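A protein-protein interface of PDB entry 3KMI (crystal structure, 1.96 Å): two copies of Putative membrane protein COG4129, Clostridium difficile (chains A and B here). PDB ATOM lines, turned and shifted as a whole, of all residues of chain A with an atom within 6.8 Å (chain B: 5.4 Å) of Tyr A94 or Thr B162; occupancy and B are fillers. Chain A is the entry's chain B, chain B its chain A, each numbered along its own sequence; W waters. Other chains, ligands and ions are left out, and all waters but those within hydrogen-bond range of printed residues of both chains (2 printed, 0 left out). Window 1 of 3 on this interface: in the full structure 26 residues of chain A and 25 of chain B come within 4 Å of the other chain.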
ATOM      1  N   ASP A  86       7.408  14.592 -15.688  1.00  0.00           N
ATOM      2  CA  ASP A  86       6.030  14.148 -15.846  1.00  0.00           C
ATOM      3  C   ASP A  86       5.502  14.667 -17.200  1.00  0.00           C
ATOM      4  O   ASP A  86       4.867  13.925 -17.918  1.00  0.00           O
ATOM      5  CB  ASP A  86       5.147  14.668 -14.711  1.00  0.00           C
ATOM      6  CG  ASP A  86       5.470  14.021 -13.343  1.00  0.00           C
ATOM      7  OD1 ASP A  86       6.209  13.021 -13.292  1.00  0.00           O
ATOM      8  OD2 ASP A  86       4.984  14.538 -12.320  1.00  0.00           O
ATOM      9  N   ILE A  87       5.748  15.936 -17.532  1.00  0.00           N
ATOM     10  CA  ILE A  87       5.356  16.454 -18.839  1.00  0.00           C
ATOM     11  C   ILE A  87       5.964  15.602 -19.990  1.00  0.00           C
ATOM     12  O   ILE A  87       5.274  15.275 -20.970  1.00  0.00           O
ATOM     13  CB  ILE A  87       5.698  17.967 -18.971  1.00  0.00           C
ATOM     14  CG1 ILE A  87       4.800  18.798 -18.046  1.00  0.00           C
ATOM     15  CG2 ILE A  87       5.650  18.424 -20.462  1.00  0.00           C
ATOM     16  CD1 ILE A  87       5.338  20.219 -17.787  1.00  0.00           C
ATOM     17  N   GLU A  89       6.808  12.459 -19.961  1.00  0.00           N
ATOM     18  CA  GLU A  89       6.084  11.180 -20.004  1.00  0.00           C
ATOM     19  C   GLU A  89       4.696  11.364 -20.619  1.00  0.00           C
ATOM     20  O   GLU A  89       4.232  10.502 -21.399  1.00  0.00           O
ATOM     21  CB  GLU A  89       5.980  10.565 -18.611  1.00  0.00           C
ATOM     22  CG  GLU A  89       7.346  10.223 -18.033  1.00  0.00           C
ATOM     23  CD  GLU A  89       7.289   9.601 -16.632  1.00  0.00           C
ATOM     24  OE1 GLU A  89       6.290   9.795 -15.888  1.00  0.00           O
ATOM     25  OE2 GLU A  89       8.278   8.934 -16.279  1.00  0.00           O
ATOM     26  N   ASN A  90       4.048  12.490 -20.303  1.00  0.00           N
ATOM     27  CA  ASN A  90       2.753  12.818 -20.907  1.00  0.00           C
ATOM     28  C   ASN A  90       2.912  12.997 -22.426  1.00  0.00           C
ATOM     29  O   ASN A  90       2.138  12.429 -23.234  1.00  0.00           O
ATOM     30  CB  ASN A  90       2.120  14.085 -20.285  1.00  0.00           C
ATOM     31  CG  ASN A  90       1.826  13.946 -18.789  1.00  0.00           C
ATOM     32  OD1 ASN A  90       1.796  12.850 -18.255  1.00  0.00           O
ATOM     33  ND2 ASN A  90       1.539  15.073 -18.121  1.00  0.00           N
ATOM     34  N   LEU A  91       3.921  13.770 -22.807  1.00  0.00           N
ATOM     35  CA  LEU A  91       4.184  14.028 -24.247  1.00  0.00           C
ATOM     36  C   LEU A  91       4.464  12.686 -24.960  1.00  0.00           C
ATOM     37  O   LEU A  91       3.955  12.427 -26.056  1.00  0.00           O
ATOM     38  CB  LEU A  91       5.345  15.032 -24.428  1.00  0.00           C
ATOM     39  CG  LEU A  91       5.129  16.507 -24.043  1.00  0.00           C
ATOM     40  CD1 LEU A  91       6.425  17.270 -24.081  1.00  0.00           C
ATOM     41  CD2 LEU A  91       4.173  17.092 -25.029  1.00  0.00           C
ATOM     42  N   TYR A  92       5.209  11.792 -24.316  1.00  0.00           N
ATOM     43  CA  TYR A  92       5.484  10.489 -24.956  1.00  0.00           C
ATOM     44  C   TYR A  92       4.192   9.683 -25.176  1.00  0.00           C
ATOM     45  O   TYR A  92       4.023   9.080 -26.232  1.00  0.00           O
ATOM     46  CB  TYR A  92       6.484   9.661 -24.145  1.00  0.00           C
ATOM     47  CG  TYR A  92       6.732   8.256 -24.697  1.00  0.00           C
ATOM     48  CD1 TYR A  92       7.646   8.045 -25.738  1.00  0.00           C
ATOM     49  CD2 TYR A  92       6.059   7.135 -24.161  1.00  0.00           C
ATOM     50  CE1 TYR A  92       7.881   6.735 -26.272  1.00  0.00           C
ATOM     51  CE2 TYR A  92       6.289   5.845 -24.661  1.00  0.00           C
ATOM     52  CZ  TYR A  92       7.193   5.653 -25.711  1.00  0.00           C
ATOM     53  OH  TYR A  92       7.408   4.394 -26.191  1.00  0.00           O
ATOM     54  N   SER A  93       3.287   9.698 -24.195  1.00  0.00           N
ATOM     55  CA  SER A  93       2.013   8.953 -24.263  1.00  0.00           C
ATOM     56  C   SER A  93       1.186   9.467 -25.437  1.00  0.00           C
ATOM     57  O   SER A  93       0.428   8.719 -26.025  1.00  0.00           O
ATOM     58  CB  SER A  93       1.193   9.093 -22.967  1.00  0.00           C
ATOM     59  OG  SER A  93       0.547  10.369 -22.943  1.00  0.00           O
ATOM     60  N   TYR A  94       1.352  10.740 -25.784  1.00  0.00           N
ATOM     61  CA  TYR A  94       0.599  11.332 -26.901  1.00  0.00           C
ATOM     62  C   TYR A  94       1.291  11.050 -28.240  1.00  0.00           C
ATOM     63  O   TYR A  94       0.692  10.529 -29.160  1.00  0.00           O
ATOM     64  CB  TYR A  94       0.463  12.849 -26.751  1.00  0.00           C
ATOM     65  CG  TYR A  94      -0.070  13.358 -25.426  1.00  0.00           C
ATOM     66  CD1 TYR A  94      -1.096  12.691 -24.742  1.00  0.00           C
ATOM     67  CD2 TYR A  94       0.424  14.551 -24.887  1.00  0.00           C
ATOM     68  CE1 TYR A  94      -1.612  13.200 -23.529  1.00  0.00           C
ATOM     69  CE2 TYR A  94      -0.085  15.069 -23.694  1.00  0.00           C
ATOM     70  CZ  TYR A  94      -1.081  14.387 -23.016  1.00  0.00           C
ATOM     71  OH  TYR A  94      -1.545  14.902 -21.827  1.00  0.00           O
ATOM     72  N   VAL A  95       2.570  11.394 -28.354  1.00  0.00           N
ATOM     73  CA  VAL A  95       3.213  11.294 -29.690  1.00  0.00           C
ATOM     74  C   VAL A  95       3.362   9.830 -30.119  1.00  0.00           C
ATOM     75  O   VAL A  95       3.392   9.504 -31.319  1.00  0.00           O
ATOM     76  CB  VAL A  95       4.564  12.032 -29.778  1.00  0.00           C
ATOM     77  CG1 VAL A  95       4.391  13.517 -29.453  1.00  0.00           C
ATOM     78  CG2 VAL A  95       5.615  11.370 -28.897  1.00  0.00           C
ATOM     79  N   SER A  96       3.407   8.922 -29.157  1.00  0.00           N
ATOM     80  CA  SER A  96       3.542   7.512 -29.549  1.00  0.00           C
ATOM     81  C   SER A  96       2.258   6.905 -30.159  1.00  0.00           C
ATOM     82  O   SER A  96       2.267   5.752 -30.631  1.00  0.00           O
ATOM     83  CB  SER A  96       4.159   6.649 -28.432  1.00  0.00           C
ATOM     84  OG  SER A  96       3.287   6.503 -27.344  1.00  0.00           O
ATOM     85  N   GLN A  97       1.187   7.693 -30.183  1.00  0.00           N
ATOM     86  CA  GLN A  97      -0.064   7.278 -30.825  1.00  0.00           C
ATOM     87  C   GLN A  97      -0.196   7.766 -32.268  1.00  0.00           C
ATOM     88  O   GLN A  97      -1.154   7.417 -32.952  1.00  0.00           O
ATOM     89  CB  GLN A  97      -1.263   7.770 -30.022  1.00  0.00           C
ATOM     90  CG  GLN A  97      -1.050   7.679 -28.519  1.00  0.00           C
ATOM     91  CD  GLN A  97      -2.217   7.054 -27.811  1.00  0.00           C
ATOM     92  OE1 GLN A  97      -3.278   6.863 -28.407  1.00  0.00           O
ATOM     93  NE2 GLN A  97      -2.031   6.712 -26.535  1.00  0.00           N
ATOM     94  N   LEU A  98       0.768   8.560 -32.725  1.00  0.00           N
ATOM     95  CA  LEU A  98       0.678   9.229 -34.034  1.00  0.00           C
ATOM     96  C   LEU A  98       0.559   8.202 -35.132  1.00  0.00           C
ATOM     97  O   LEU A  98       1.324   7.230 -35.155  1.00  0.00           O
ATOM     98  CB  LEU A  98       1.880  10.160 -34.286  1.00  0.00           C
ATOM     99  CG  LEU A  98       1.752  11.548 -33.628  1.00  0.00           C
ATOM    100  CD1 LEU A  98       3.116  12.233 -33.615  1.00  0.00           C
ATOM    101  CD2 LEU A  98       0.676  12.447 -34.303  1.00  0.00           C
ATOM    102  N   ALA A 155      -5.662  16.100 -32.468  1.00  0.00           N
ATOM    103  CA  ALA A 155      -5.845  16.007 -31.031  1.00  0.00           C
ATOM    104  C   ALA A 155      -4.487  15.854 -30.389  1.00  0.00           C
ATOM    105  O   ALA A 155      -4.183  16.559 -29.430  1.00  0.00           O
ATOM    106  CB  ALA A 155      -6.740  14.822 -30.667  1.00  0.00           C
ATOM    107  N   ILE A 156      -3.659  14.952 -30.921  1.00  0.00           N
ATOM    108  CA  ILE A 156      -2.357  14.697 -30.303  1.00  0.00           C
ATOM    109  C   ILE A 156      -1.470  15.947 -30.317  1.00  0.00           C
ATOM    110  O   ILE A 156      -0.780  16.240 -29.338  1.00  0.00           O
ATOM    111  CB  ILE A 156      -1.603  13.526 -30.996  1.00  0.00           C
ATOM    112  CG1 ILE A 156      -2.242  12.193 -30.608  1.00  0.00           C
ATOM    113  CG2 ILE A 156      -0.120  13.542 -30.614  1.00  0.00           C
ATOM    114  CD1 ILE A 156      -2.084  11.156 -31.682  1.00  0.00           C
ATOM    115  N   LEU A 157      -1.484  16.677 -31.430  1.00  0.00           N
ATOM    116  CA  LEU A 157      -0.679  17.900 -31.557  1.00  0.00           C
ATOM    117  C   LEU A 157      -1.156  19.023 -30.637  1.00  0.00           C
ATOM    118  O   LEU A 157      -0.350  19.792 -30.098  1.00  0.00           O
ATOM    119  CB  LEU A 157      -0.663  18.376 -33.033  1.00  0.00           C
ATOM    120  CG  LEU A 157       0.003  17.416 -34.003  1.00  0.00           C
ATOM    121  CD1 LEU A 157      -0.069  17.933 -35.480  1.00  0.00           C
ATOM    122  CD2 LEU A 157       1.448  17.199 -33.623  1.00  0.00           C
ATOM    123  N   LEU A 159      -2.800  18.505 -27.715  1.00  0.00           N
ATOM    124  CA  LEU A 159      -2.412  18.087 -26.356  1.00  0.00           C
ATOM    125  C   LEU A 159      -0.923  18.403 -26.139  1.00  0.00           C
ATOM    126  O   LEU A 159      -0.524  18.905 -25.070  1.00  0.00           O
ATOM    127  CB  LEU A 159      -2.669  16.587 -26.175  1.00  0.00           C
ATOM    128  CG  LEU A 159      -4.101  16.077 -26.360  1.00  0.00           C
ATOM    129  CD1 LEU A 159      -4.160  14.540 -26.334  1.00  0.00           C
ATOM    130  CD2 LEU A 159      -4.967  16.622 -25.299  1.00  0.00           C
ATOM    131  N   CYS A 160      -0.094  18.094 -27.130  1.00  0.00           N
ATOM    132  CA  CYS A 160       1.343  18.441 -27.042  1.00  0.00           C
ATOM    133  C   CYS A 160       1.635  19.948 -26.869  1.00  0.00           C
ATOM    134  O   CYS A 160       2.467  20.299 -26.047  1.00  0.00           O
ATOM    135  CB  CYS A 160       2.126  17.932 -28.254  1.00  0.00           C
ATOM    136  SG  CYS A 160       2.276  16.122 -28.353  1.00  0.00           S
ATOM    137  N   GLU A 163       0.754  21.000 -23.256  1.00  0.00           N
ATOM    138  CA  GLU A 163       1.763  20.626 -22.248  1.00  0.00           C
ATOM    139  C   GLU A 163       3.096  21.363 -22.420  1.00  0.00           C
ATOM    140  O   GLU A 163       3.770  21.657 -21.438  1.00  0.00           O
ATOM    141  CB  GLU A 163       1.989  19.102 -22.296  1.00  0.00           C
ATOM    142  CG  GLU A 163       0.712  18.329 -22.015  1.00  0.00           C
ATOM    143  CD  GLU A 163       0.728  17.553 -20.724  1.00  0.00           C
ATOM    144  OE1 GLU A 163       1.597  17.778 -19.866  1.00  0.00           O
ATOM    145  OE2 GLU A 163      -0.109  16.651 -20.581  1.00  0.00           O
ATOM    146  N   MET B 136     -10.618   6.550 -21.472  1.00  0.00           N
ATOM    147  CA  MET B 136      -9.750   7.117 -22.518  1.00  0.00           C
ATOM    148  C   MET B 136     -10.167   6.543 -23.876  1.00  0.00           C
ATOM    149  O   MET B 136     -10.334   7.289 -24.843  1.00  0.00           O
ATOM    150  CB  MET B 136      -8.251   6.821 -22.265  1.00  0.00           C
ATOM    151  CG  MET B 136      -7.607   7.440 -20.997  1.00  0.00           C
ATOM    152  SD  MET B 136      -5.636   7.320 -20.973  1.00  0.00           S
ATOM    153  CE  MET B 136      -5.256   8.428 -19.362  1.00  0.00           C
ATOM    154  N   PHE B 158      -9.546  15.118 -22.036  1.00  0.00           N
ATOM    155  CA  PHE B 158      -8.514  14.097 -22.208  1.00  0.00           C
ATOM    156  C   PHE B 158      -7.250  14.403 -21.383  1.00  0.00           C
ATOM    157  O   PHE B 158      -6.584  13.484 -20.889  1.00  0.00           O
ATOM    158  CB  PHE B 158      -8.156  13.908 -23.684  1.00  0.00           C
ATOM    159  CG  PHE B 158      -7.467  12.609 -23.965  1.00  0.00           C
ATOM    160  CD1 PHE B 158      -8.204  11.441 -24.122  1.00  0.00           C
ATOM    161  CD2 PHE B 158      -6.091  12.546 -24.052  1.00  0.00           C
ATOM    162  CE1 PHE B 158      -7.580  10.237 -24.363  1.00  0.00           C
ATOM    163  CE2 PHE B 158      -5.452  11.344 -24.299  1.00  0.00           C
ATOM    164  CZ  PHE B 158      -6.201  10.186 -24.460  1.00  0.00           C
ATOM    165  N   LEU B 159      -6.932  15.688 -21.240  1.00  0.00           N
ATOM    166  CA  LEU B 159      -5.793  16.105 -20.395  1.00  0.00           C
ATOM    167  C   LEU B 159      -6.042  15.784 -18.922  1.00  0.00           C
ATOM    168  O   LEU B 159      -5.081  15.488 -18.168  1.00  0.00           O
ATOM    169  CB  LEU B 159      -5.467  17.600 -20.567  1.00  0.00           C
ATOM    170  CG  LEU B 159      -4.918  18.086 -21.915  1.00  0.00           C
ATOM    171  CD1 LEU B 159      -5.321  19.523 -22.170  1.00  0.00           C
ATOM    172  CD2 LEU B 159      -3.437  17.893 -21.990  1.00  0.00           C
ATOM    173  N   CYS B 160      -7.312  15.876 -18.520  1.00  0.00           N
ATOM    174  CA  CYS B 160      -7.728  15.410 -17.169  1.00  0.00           C
ATOM    175  C   CYS B 160      -7.396  13.932 -16.920  1.00  0.00           C
ATOM    176  O   CYS B 160      -6.876  13.586 -15.861  1.00  0.00           O
ATOM    177  CB  CYS B 160      -9.197  15.673 -16.949  1.00  0.00           C
ATOM    178  SG  CYS B 160      -9.517  17.430 -16.724  1.00  0.00           S
ATOM    179  N   LEU B 161      -7.672  13.074 -17.911  1.00  0.00           N
ATOM    180  CA  LEU B 161      -7.371  11.643 -17.795  1.00  0.00           C
ATOM    181  C   LEU B 161      -5.874  11.395 -17.629  1.00  0.00           C
ATOM    182  O   LEU B 161      -5.458  10.504 -16.853  1.00  0.00           O
ATOM    183  CB  LEU B 161      -7.911  10.851 -19.005  1.00  0.00           C
ATOM    184  CG  LEU B 161      -9.420  10.964 -19.233  1.00  0.00           C
ATOM    185  CD1 LEU B 161      -9.855  10.029 -20.341  1.00  0.00           C
ATOM    186  CD2 LEU B 161     -10.154  10.658 -17.951  1.00  0.00           C
ATOM    187  N   THR B 162      -5.062  12.197 -18.323  1.00  0.00           N
ATOM    188  CA  THR B 162      -3.614  12.108 -18.163  1.00  0.00           C
ATOM    189  C   THR B 162      -3.206  12.362 -16.726  1.00  0.00           C
ATOM    190  O   THR B 162      -2.430  11.598 -16.153  1.00  0.00           O
ATOM    191  CB  THR B 162      -2.862  13.057 -19.129  1.00  0.00           C
ATOM    192  OG1 THR B 162      -3.144  12.650 -20.478  1.00  0.00           O
ATOM    193  CG2 THR B 162      -1.409  12.952 -18.906  1.00  0.00           C
ATOM    194  N   GLU B 163      -3.723  13.428 -16.147  1.00  0.00           N
ATOM    195  CA  GLU B 163      -3.400  13.790 -14.759  1.00  0.00           C
ATOM    196  C   GLU B 163      -3.915  12.715 -13.788  1.00  0.00           C
ATOM    197  O   GLU B 163      -3.201  12.286 -12.867  1.00  0.00           O
ATOM    198  CB  GLU B 163      -3.987  15.165 -14.400  1.00  0.00           C
ATOM    199  CG  GLU B 163      -3.362  16.311 -15.196  1.00  0.00           C
ATOM    200  CD  GLU B 163      -1.842  16.444 -14.989  1.00  0.00           C
ATOM    201  OE1 GLU B 163      -1.318  16.263 -13.860  1.00  0.00           O
ATOM    202  OE2 GLU B 163      -1.157  16.741 -15.983  1.00  0.00           O
ATOM    203  N   LEU B 164      -5.120  12.223 -14.048  1.00  0.00           N
ATOM    204  CA  LEU B 164      -5.706  11.205 -13.200  1.00  0.00           C
ATOM    205  C   LEU B 164      -4.930   9.895 -13.188  1.00  0.00           C
ATOM    206  O   LEU B 164      -4.935   9.194 -12.184  1.00  0.00           O
ATOM    207  CB  LEU B 164      -7.179  10.952 -13.568  1.00  0.00           C
ATOM    208  CG  LEU B 164      -8.162  12.046 -13.147  1.00  0.00           C
ATOM    209  CD1 LEU B 164      -9.553  11.622 -13.721  1.00  0.00           C
ATOM    210  CD2 LEU B 164      -8.262  12.162 -11.592  1.00  0.00           C
ATOM    211  N   LYS B 165      -4.277   9.537 -14.282  1.00  0.00           N
ATOM    212  CA  LYS B 165      -3.492   8.304 -14.295  1.00  0.00           C
ATOM    213  C   LYS B 165      -2.349   8.429 -13.297  1.00  0.00           C
ATOM    214  O   LYS B 165      -2.109   7.529 -12.502  1.00  0.00           O
ATOM    215  CB  LYS B 165      -2.943   7.994 -15.695  1.00  0.00           C
ATOM    216  CG  LYS B 165      -2.338   6.608 -15.823  1.00  0.00           C
ATOM    217  CD  LYS B 165      -1.871   6.364 -17.266  1.00  0.00           C
ATOM    218  CE  LYS B 165      -1.308   4.977 -17.466  1.00  0.00           C
ATOM    219  NZ  LYS B 165      -1.025   4.796 -18.899  1.00  0.00           N
ATOM    220  N   GLN B 166      -1.637   9.550 -13.349  1.00  0.00           N
ATOM    221  CA  GLN B 166      -0.542   9.758 -12.397  1.00  0.00           C
ATOM    222  C   GLN B 166      -1.052   9.873 -10.967  1.00  0.00           C
ATOM    223  O   GLN B 166      -0.427   9.349 -10.078  1.00  0.00           O
ATOM    224  CB  GLN B 166       0.333  10.951 -12.744  1.00  0.00           C
ATOM    225  CG  GLN B 166       1.653  10.873 -11.921  1.00  0.00           C
ATOM    226  CD  GLN B 166       2.449   9.543 -12.143  1.00  0.00           C
ATOM    227  OE1 GLN B 166       2.705   9.123 -13.286  1.00  0.00           O
ATOM    228  NE2 GLN B 166       2.855   8.908 -11.042  1.00  0.00           N
HETATM  229  O   HOH W   1      -1.828  16.928 -18.505  1.00  0.00           O
HETATM  230  O   HOH W   2       1.657  16.700 -15.772  1.00  0.00           O
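Leu A159 touches its own counterpart, Leu B159. Glu A163 touches Leu B159, but with the chains exchanged Leu A159 does not touch Glu B163 (9.4 Å).
Among the printed residues, merely in contact across the chains: Asn A90 with Thr B162 (3.3 Å), Asn A90 with Glu B163 (3.8 Å), Tyr A94 with Leu B159 (3.5 Å), Leu A159 with Phe B158 (3.6 Å), Leu A159 with Leu B159 (3.7 Å) and Glu A163 with Leu B159 (3.8 Å).
The side-chain carboxylate (OE1) of Glu A163 lies within hydrogen-bond range of the side-chain amide nitrogen (ND2) of Asn A90, 3.2 Å away. The side-chain hydroxyl of Tyr A94 is in hydrogen-bond range of the side-chain carboxylate of Glu A163 (2.6 Å). The side-chain amide oxygen (OD1) of Asn A90 sits close to the backbone carbonyl oxygen (O) of Asp A86 (3.3 Å). O of Asn A90 lies within hydrogen-bond range of OG of Ser A93 (2.6 Å).
Printed residues of chain B that touch a printed residue of chain A: Phe B158, Leu B159, Thr B162 and Glu B163. Among the printed residues, 7 pairs touch across the chains. Among the printed residues, no Asp or Glu carboxylate lies within 4 Å of a Lys or Arg side-chain nitrogen of the other chain.
Of chain B, only Leu B159 (3.5 Å) and Thr B162 (3.1 Å) come within 4 Å of Tyr A94. Of chain A, only Asn A90 (3.3 Å) and Tyr A94 (3.1 Å) come within 4 Å of Thr B162. Of the printed residues of chain B, Leu A159 touches Phe B158 (3.6 Å) and Leu B159 (3.7 Å). Printed residues of chain A within 4 Å of Phe B158: Leu A159. Of the printed residues of chain B, Asn A90 touches Thr B162 and Glu B163. Of the printed residues of chain A, Glu B163 touches Asn A90. Gln A97 touches none of the printed residues of chain B. Ala A155 touches none of the printed residues of chain B.
The side-chain hydroxyl (OG1) of Thr B162 sits at hydrogen-bond distance from the side-chain hydroxyl (OH) of Tyr A94 (3.1 Å).
Water W1 bridges OE2 of Glu B163 (2.6 Å) and OE2 of Glu A163 (2.7 Å). Water W2 bridges the side-chain carboxylate (OE2) of Glu B163 (2.8 Å) and the side-chain amide nitrogen (ND2) of Asn A90 (2.9 Å).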
